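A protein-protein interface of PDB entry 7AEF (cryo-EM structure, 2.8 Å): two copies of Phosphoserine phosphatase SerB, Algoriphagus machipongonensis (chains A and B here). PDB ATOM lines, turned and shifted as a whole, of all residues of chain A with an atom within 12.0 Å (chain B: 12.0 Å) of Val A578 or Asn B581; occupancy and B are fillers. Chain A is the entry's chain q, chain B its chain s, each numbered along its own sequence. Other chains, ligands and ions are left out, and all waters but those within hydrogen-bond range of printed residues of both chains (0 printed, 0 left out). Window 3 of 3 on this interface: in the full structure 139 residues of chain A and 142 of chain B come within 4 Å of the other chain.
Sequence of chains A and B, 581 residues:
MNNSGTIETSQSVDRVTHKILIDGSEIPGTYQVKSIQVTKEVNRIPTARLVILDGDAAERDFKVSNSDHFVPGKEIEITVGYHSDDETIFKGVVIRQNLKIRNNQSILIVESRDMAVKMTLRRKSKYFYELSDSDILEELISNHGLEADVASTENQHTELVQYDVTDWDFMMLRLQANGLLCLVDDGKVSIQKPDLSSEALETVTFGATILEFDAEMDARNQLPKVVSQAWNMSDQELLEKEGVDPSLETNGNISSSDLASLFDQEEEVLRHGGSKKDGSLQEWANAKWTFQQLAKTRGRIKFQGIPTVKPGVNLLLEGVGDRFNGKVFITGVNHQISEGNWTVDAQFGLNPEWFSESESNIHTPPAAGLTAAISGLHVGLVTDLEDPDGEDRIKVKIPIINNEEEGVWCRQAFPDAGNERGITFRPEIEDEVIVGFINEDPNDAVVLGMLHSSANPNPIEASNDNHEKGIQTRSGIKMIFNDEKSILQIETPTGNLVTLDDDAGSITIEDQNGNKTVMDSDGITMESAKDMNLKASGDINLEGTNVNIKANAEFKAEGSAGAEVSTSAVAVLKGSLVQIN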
ATOM      1  N   VAL A 570      11.842  15.004  23.951  1.00  0.00           N
ATOM      2  CA  VAL A 570      12.136  14.023  24.995  1.00  0.00           C
ATOM      3  C   VAL A 570      13.000  12.882  24.501  1.00  0.00           C
ATOM      4  O   VAL A 570      12.640  12.220  23.531  1.00  0.00           O
ATOM      5  CB  VAL A 570      10.825  13.421  25.553  1.00  0.00           C
ATOM      6  CG1 VAL A 570      11.129  12.401  26.643  1.00  0.00           C
ATOM      7  CG2 VAL A 570       9.936  14.514  26.096  1.00  0.00           C
ATOM      8  N   ALA A 571      14.109  12.612  25.174  1.00  0.00           N
ATOM      9  CA  ALA A 571      14.934  11.473  24.800  1.00  0.00           C
ATOM     10  C   ALA A 571      14.523  10.290  25.660  1.00  0.00           C
ATOM     11  O   ALA A 571      14.268  10.458  26.850  1.00  0.00           O
ATOM     12  CB  ALA A 571      16.397  11.791  24.970  1.00  0.00           C
ATOM     13  N   VAL A 572      14.451   9.100  25.075  1.00  0.00           N
ATOM     14  CA  VAL A 572      14.056   7.911  25.821  1.00  0.00           C
ATOM     15  C   VAL A 572      14.999   6.726  25.653  1.00  0.00           C
ATOM     16  O   VAL A 572      15.298   6.327  24.533  1.00  0.00           O
ATOM     17  CB  VAL A 572      12.638   7.485  25.389  1.00  0.00           C
ATOM     18  CG1 VAL A 572      12.216   6.241  26.107  1.00  0.00           C
ATOM     19  CG2 VAL A 572      11.662   8.602  25.678  1.00  0.00           C
ATOM     20  N   LEU A 573      15.431   6.146  26.770  1.00  0.00           N
ATOM     21  CA  LEU A 573      16.271   4.954  26.755  1.00  0.00           C
ATOM     22  C   LEU A 573      15.637   3.863  27.612  1.00  0.00           C
ATOM     23  O   LEU A 573      15.512   4.022  28.823  1.00  0.00           O
ATOM     24  CB  LEU A 573      17.673   5.305  27.263  1.00  0.00           C
ATOM     25  CG  LEU A 573      18.700   4.158  27.415  1.00  0.00           C
ATOM     26  CD1 LEU A 573      18.989   3.517  26.084  1.00  0.00           C
ATOM     27  CD2 LEU A 573      19.978   4.727  27.999  1.00  0.00           C
ATOM     28  N   LYS A 574      15.205   2.779  26.991  1.00  0.00           N
ATOM     29  CA  LYS A 574      14.601   1.690  27.738  1.00  0.00           C
ATOM     30  C   LYS A 574      14.988   0.287  27.316  1.00  0.00           C
ATOM     31  O   LYS A 574      15.333   0.027  26.211  1.00  0.00           O
ATOM     32  CB  LYS A 574      13.094   1.862  27.900  1.00  0.00           C
ATOM     33  CG  LYS A 574      12.258   1.711  26.666  1.00  0.00           C
ATOM     34  CD  LYS A 574      10.810   1.912  27.041  1.00  0.00           C
ATOM     35  CE  LYS A 574       9.896   1.549  25.886  1.00  0.00           C
ATOM     36  NZ  LYS A 574       9.010   2.674  25.486  1.00  0.00           N
ATOM     37  N   GLY A 575      14.903  -0.614  28.257  1.00  0.00           N
ATOM     38  CA  GLY A 575      15.301  -2.000  28.117  1.00  0.00           C
ATOM     39  C   GLY A 575      14.994  -2.698  29.419  1.00  0.00           C
ATOM     40  O   GLY A 575      14.614  -2.046  30.387  1.00  0.00           O
ATOM     41  N   SER A 576      15.159  -4.021  29.464  1.00  0.00           N
ATOM     42  CA  SER A 576      14.910  -4.776  30.695  1.00  0.00           C
ATOM     43  C   SER A 576      16.027  -4.548  31.704  1.00  0.00           C
ATOM     44  O   SER A 576      15.886  -4.823  32.895  1.00  0.00           O
ATOM     45  CB  SER A 576      14.788  -6.245  30.382  1.00  0.00           C
ATOM     46  OG  SER A 576      16.009  -6.755  29.937  1.00  0.00           O
ATOM     47  N   LEU A 577      17.126  -4.029  31.191  1.00  0.00           N
ATOM     48  CA  LEU A 577      18.325  -3.680  31.908  1.00  0.00           C
ATOM     49  C   LEU A 577      19.084  -2.640  31.117  1.00  0.00           C
ATOM     50  O   LEU A 577      19.377  -2.840  29.939  1.00  0.00           O
ATOM     51  CB  LEU A 577      19.214  -4.903  32.121  1.00  0.00           C
ATOM     52  CG  LEU A 577      20.581  -4.653  32.819  1.00  0.00           C
ATOM     53  CD1 LEU A 577      20.380  -4.209  34.249  1.00  0.00           C
ATOM     54  CD2 LEU A 577      21.398  -5.908  32.761  1.00  0.00           C
ATOM     55  N   VAL A 578      19.422  -1.539  31.751  1.00  0.00           N
ATOM     56  CA  VAL A 578      20.185  -0.504  31.084  1.00  0.00           C
ATOM     57  C   VAL A 578      21.520  -0.331  31.765  1.00  0.00           C
ATOM     58  O   VAL A 578      21.583  -0.103  32.968  1.00  0.00           O
ATOM     59  CB  VAL A 578      19.407   0.829  31.067  1.00  0.00           C
ATOM     60  CG1 VAL A 578      20.244   1.926  30.427  1.00  0.00           C
ATOM     61  CG2 VAL A 578      18.102   0.650  30.272  1.00  0.00           C
ATOM     62  N   GLN A 579      22.588  -0.443  30.992  1.00  0.00           N
ATOM     63  CA  GLN A 579      23.926  -0.283  31.530  1.00  0.00           C
ATOM     64  C   GLN A 579      24.614   0.899  30.891  1.00  0.00           C
ATOM     65  O   GLN A 579      24.511   1.103  29.685  1.00  0.00           O
ATOM     66  CB  GLN A 579      24.757  -1.533  31.286  1.00  0.00           C
ATOM     67  CG  GLN A 579      24.236  -2.760  31.968  1.00  0.00           C
ATOM     68  CD  GLN A 579      25.112  -3.943  31.733  1.00  0.00           C
ATOM     69  OE1 GLN A 579      25.648  -4.114  30.639  1.00  0.00           O
ATOM     70  NE2 GLN A 579      25.279  -4.773  32.748  1.00  0.00           N
ATOM     71  N   ILE A 580      25.332   1.660  31.700  1.00  0.00           N
ATOM     72  CA  ILE A 580      26.089   2.800  31.226  1.00  0.00           C
ATOM     73  C   ILE A 580      27.533   2.643  31.658  1.00  0.00           C
ATOM     74  O   ILE A 580      27.815   2.507  32.844  1.00  0.00           O
ATOM     75  CB  ILE A 580      25.478   4.107  31.753  1.00  0.00           C
ATOM     76  CG1 ILE A 580      24.003   4.204  31.250  1.00  0.00           C
ATOM     77  CG2 ILE A 580      26.314   5.296  31.297  1.00  0.00           C
ATOM     78  CD1 ILE A 580      23.188   5.312  31.829  1.00  0.00           C
ATOM     79  N   ASN A 581      28.455   2.654  30.706  1.00  0.00           N
ATOM     80  CA  ASN A 581      29.865   2.453  31.012  1.00  0.00           C
ATOM     81  C   ASN A 581      30.052   1.415  32.104  1.00  0.00           C
ATOM     82  O   ASN A 581      30.635   0.355  31.865  1.00  0.00           O
ATOM     83  CB  ASN A 581      30.543   3.742  31.399  1.00  0.00           C
ATOM     84  CG  ASN A 581      30.696   4.646  30.266  1.00  0.00           C
ATOM     85  OD1 ASN A 581      30.677   4.221  29.106  1.00  0.00           O
ATOM     86  ND2 ASN A 581      30.859   5.899  30.551  1.00  0.00           N
ATOM     87  N   ALA B 557      14.191   3.732  16.882  1.00  0.00           N
ATOM     88  CA  ALA B 557      15.010   2.583  16.571  1.00  0.00           C
ATOM     89  C   ALA B 557      14.685   1.505  17.576  1.00  0.00           C
ATOM     90  O   ALA B 557      14.517   1.792  18.759  1.00  0.00           O
ATOM     91  CB  ALA B 557      16.473   2.948  16.600  1.00  0.00           C
ATOM     92  N   GLY B 559      15.126  -2.979  18.630  1.00  0.00           N
ATOM     93  CA  GLY B 559      15.708  -4.285  18.406  1.00  0.00           C
ATOM     94  C   GLY B 559      15.122  -5.253  19.414  1.00  0.00           C
ATOM     95  O   GLY B 559      15.204  -5.041  20.624  1.00  0.00           O
ATOM     96  N   ALA B 561      16.239  -8.042  20.340  1.00  0.00           N
ATOM     97  CA  ALA B 561      17.266  -8.704  21.104  1.00  0.00           C
ATOM     98  C   ALA B 561      18.274  -7.696  21.617  1.00  0.00           C
ATOM     99  O   ALA B 561      19.418  -8.051  21.898  1.00  0.00           O
ATOM    100  CB  ALA B 561      17.947  -9.758  20.265  1.00  0.00           C
ATOM    101  N   GLY B 562      17.854  -6.443  21.764  1.00  0.00           N
ATOM    102  CA  GLY B 562      18.745  -5.421  22.281  1.00  0.00           C
ATOM    103  C   GLY B 562      19.194  -4.415  21.243  1.00  0.00           C
ATOM    104  O   GLY B 562      19.027  -4.599  20.038  1.00  0.00           O
ATOM    105  N   ALA B 563      19.792  -3.340  21.737  1.00  0.00           N
ATOM    106  CA  ALA B 563      20.268  -2.246  20.922  1.00  0.00           C
ATOM    107  C   ALA B 563      21.482  -1.647  21.588  1.00  0.00           C
ATOM    108  O   ALA B 563      21.628  -1.742  22.802  1.00  0.00           O
ATOM    109  CB  ALA B 563      19.177  -1.209  20.740  1.00  0.00           C
ATOM    110  N   GLU B 564      22.347  -1.029  20.802  1.00  0.00           N
ATOM    111  CA  GLU B 564      23.558  -0.433  21.334  1.00  0.00           C
ATOM    112  C   GLU B 564      24.027   0.780  20.573  1.00  0.00           C
ATOM    113  O   GLU B 564      24.011   0.803  19.345  1.00  0.00           O
ATOM    114  CB  GLU B 564      24.677  -1.472  21.322  1.00  0.00           C
ATOM    115  CG  GLU B 564      26.008  -0.994  21.862  1.00  0.00           C
ATOM    116  CD  GLU B 564      27.037  -2.071  21.899  1.00  0.00           C
ATOM    117  OE1 GLU B 564      26.728  -3.178  21.546  1.00  0.00           O
ATOM    118  OE2 GLU B 564      28.145  -1.789  22.280  1.00  0.00           O
ATOM    119  N   VAL B 565      24.465   1.782  21.316  1.00  0.00           N
ATOM    120  CA  VAL B 565      25.079   2.972  20.767  1.00  0.00           C
ATOM    121  C   VAL B 565      26.431   3.108  21.423  1.00  0.00           C
ATOM    122  O   VAL B 565      26.518   3.153  22.646  1.00  0.00           O
ATOM    123  CB  VAL B 565      24.225   4.214  21.034  1.00  0.00           C
ATOM    124  CG1 VAL B 565      24.906   5.447  20.485  1.00  0.00           C
ATOM    125  CG2 VAL B 565      22.873   4.030  20.394  1.00  0.00           C
ATOM    126  N   ALA B 571      29.911   9.907  24.031  1.00  0.00           N
ATOM    127  CA  ALA B 571      28.519   9.635  23.699  1.00  0.00           C
ATOM    128  C   ALA B 571      27.676  10.784  24.228  1.00  0.00           C
ATOM    129  O   ALA B 571      27.927  11.273  25.326  1.00  0.00           O
ATOM    130  CB  ALA B 571      28.076   8.318  24.281  1.00  0.00           C
ATOM    131  N   LEU B 573      23.602  12.279  24.851  1.00  0.00           N
ATOM    132  CA  LEU B 573      22.151  12.129  24.858  1.00  0.00           C
ATOM    133  C   LEU B 573      21.498  13.419  25.341  1.00  0.00           C
ATOM    134  O   LEU B 573      21.677  13.811  26.490  1.00  0.00           O
ATOM    135  CB  LEU B 573      21.760  10.947  25.753  1.00  0.00           C
ATOM    136  CG  LEU B 573      20.255  10.668  25.972  1.00  0.00           C
ATOM    137  CD1 LEU B 573      19.577  10.329  24.672  1.00  0.00           C
ATOM    138  CD2 LEU B 573      20.113   9.513  26.944  1.00  0.00           C
ATOM    139  N   LEU B 577      13.831  16.905  27.867  1.00  0.00           N
ATOM    140  CA  LEU B 577      13.535  15.957  28.910  1.00  0.00           C
ATOM    141  C   LEU B 577      14.082  14.605  28.512  1.00  0.00           C
ATOM    142  O   LEU B 577      13.782  14.102  27.430  1.00  0.00           O
ATOM    143  CB  LEU B 577      12.029  15.846  29.141  1.00  0.00           C
ATOM    144  CG  LEU B 577      11.565  14.798  30.191  1.00  0.00           C
ATOM    145  CD1 LEU B 577      12.027  15.187  31.577  1.00  0.00           C
ATOM    146  CD2 LEU B 577      10.072  14.682  30.141  1.00  0.00           C
ATOM    147  N   VAL B 578      14.865  14.001  29.379  1.00  0.00           N
ATOM    148  CA  VAL B 578      15.403  12.687  29.100  1.00  0.00           C
ATOM    149  C   VAL B 578      14.889  11.696  30.115  1.00  0.00           C
ATOM    150  O   VAL B 578      15.034  11.895  31.316  1.00  0.00           O
ATOM    151  CB  VAL B 578      16.947  12.712  29.104  1.00  0.00           C
ATOM    152  CG1 VAL B 578      17.503  11.313  28.878  1.00  0.00           C
ATOM    153  CG2 VAL B 578      17.444  13.647  27.987  1.00  0.00           C
ATOM    154  N   GLN B 579      14.279  10.626  29.628  1.00  0.00           N
ATOM    155  CA  GLN B 579      13.753   9.596  30.505  1.00  0.00           C
ATOM    156  C   GLN B 579      14.456   8.284  30.257  1.00  0.00           C
ATOM    157  O   GLN B 579      14.704   7.915  29.113  1.00  0.00           O
ATOM    158  CB  GLN B 579      12.261   9.411  30.281  1.00  0.00           C
ATOM    159  CG  GLN B 579      11.435  10.618  30.604  1.00  0.00           C
ATOM    160  CD  GLN B 579       9.978  10.366  30.410  1.00  0.00           C
ATOM    161  OE1 GLN B 579       9.586   9.672  29.474  1.00  0.00           O
ATOM    162  NE2 GLN B 579       9.157  10.915  31.289  1.00  0.00           N
ATOM    163  N   ILE B 580      14.752   7.573  31.332  1.00  0.00           N
ATOM    164  CA  ILE B 580      15.383   6.271  31.253  1.00  0.00           C
ATOM    165  C   ILE B 580      14.530   5.268  32.005  1.00  0.00           C
ATOM    166  O   ILE B 580      14.254   5.448  33.186  1.00  0.00           O
ATOM    167  CB  ILE B 580      16.812   6.332  31.812  1.00  0.00           C
ATOM    168  CG1 ILE B 580      17.629   7.367  30.977  1.00  0.00           C
ATOM    169  CG2 ILE B 580      17.446   4.947  31.777  1.00  0.00           C
ATOM    170  CD1 ILE B 580      18.984   7.705  31.500  1.00  0.00           C
ATOM    171  N   ASN B 581      14.104   4.210  31.331  1.00  0.00           N
ATOM    172  CA  ASN B 581      13.232   3.218  31.945  1.00  0.00           C
ATOM    173  C   ASN B 581      12.218   3.870  32.868  1.00  0.00           C
ATOM    174  O   ASN B 581      11.012   3.804  32.618  1.00  0.00           O
ATOM    175  CB  ASN B 581      14.016   2.170  32.691  1.00  0.00           C
ATOM    176  CG  ASN B 581      14.747   1.285  31.794  1.00  0.00           C
ATOM    177  OD1 ASN B 581      14.405   1.151  30.614  1.00  0.00           O
ATOM    178  ND2 ASN B 581      15.755   0.652  32.308  1.00  0.00           N
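Val A578 touches just one residue of chain B: Asn B581. Asn B581 touches just these residues of chain A: Leu A573, Lys A574, Gly A575 and Val A578. Leu A573 touches just these residues of chain B: Gln B579 (3.0 Å), Ile B580 (3.3 Å) and Asn B581 (2.9 Å). Lys A574 touches one residue of chain B. Gly A575 touches just one residue of chain B: Asn B581 (3.0 Å). No residue of chain B comes within 4 Å of Ser A576. Gln A579 touches none of the printed residues of chain B. Gln B579 touches just these residues of chain A: Ala A571 (2.8 Å), Val A572 (3.4 Å) and Leu A573 (3.0 Å). Of the printed residues of chain A, Leu B577 touches Val A570 and Ala A571. Printed residues of chain B within 4 Å of Ala A571: Leu B573 (3.5 Å), Leu B577 (2.7 Å), Val B578 (3.4 Å) and Gln B579 (2.8 Å). The nearest residue of chain B that does not touch Val A578 is Ile B580 (4.3 Å). The nearest residue of chain A that does not touch Asn B581 is Leu A577 (4.8 Å).
Ala A571 touches Leu B573, but with the chains exchanged Leu A573 does not touch Ala B571 (9.6 Å). Ala A571 touches Leu B577, but with the chains exchanged Leu A577 does not touch Ala B571 (15.2 Å). Leu A573 touches Asn B581, but with the chains exchanged Asn A581 does not touch Leu B573 (11.2 Å). Val A578 touches Asn B581, but with the chains exchanged Asn A581 does not touch Val B578 (14.1 Å). Of the 12 pairs that touch across the chains among the printed residues, none has its exchanged pair printed and touching as well.
N of Ala A571 lies within hydrogen-bond range of O of Leu B577 (2.7 Å). The backbone carbonyl oxygen of Ala A571 sits at hydrogen-bond distance from the backbone NH of Gln B579 (2.8 Å). N of Leu A573 sits at hydrogen-bond distance from O of Gln B579 (3.0 Å). O of Leu A573 is in hydrogen-bond range of N of Asn B581, at 2.9 Å. OD1 of Asn B581 sits at hydrogen-bond distance from N of Gly A575 (3.0 Å).
Of the 12 printed residues of chain A, 7 touch a printed residue of chain B. Hydrophobic or aromatic side chains of chain A within 4 Å of the printed part of chain B: Val A570, Ala A571 and Val A578. Of the 14 printed residues of chain B, 6 touch a printed residue of chain A. Hydrophobic or aromatic side chains of chain B within 4 Å of the printed part of chain A: Leu B573, Leu B577, Val B578 and Ile B580.
Leu B577 touches Val A570 (O to CA, 2.9 Å). Leu B573 touches Ala A571 (CD1 to CB, 3.5 Å). O of Ala A571 touches CA of Val B578 (3.4 Å). Gln B579 touches Val A572. Ile B580 touches Leu A573 (CA to O, 3.3 Å). CA of Lys A574 touches OD1 of Asn B581, 2.9 Å away. Val A578 touches Asn B581.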
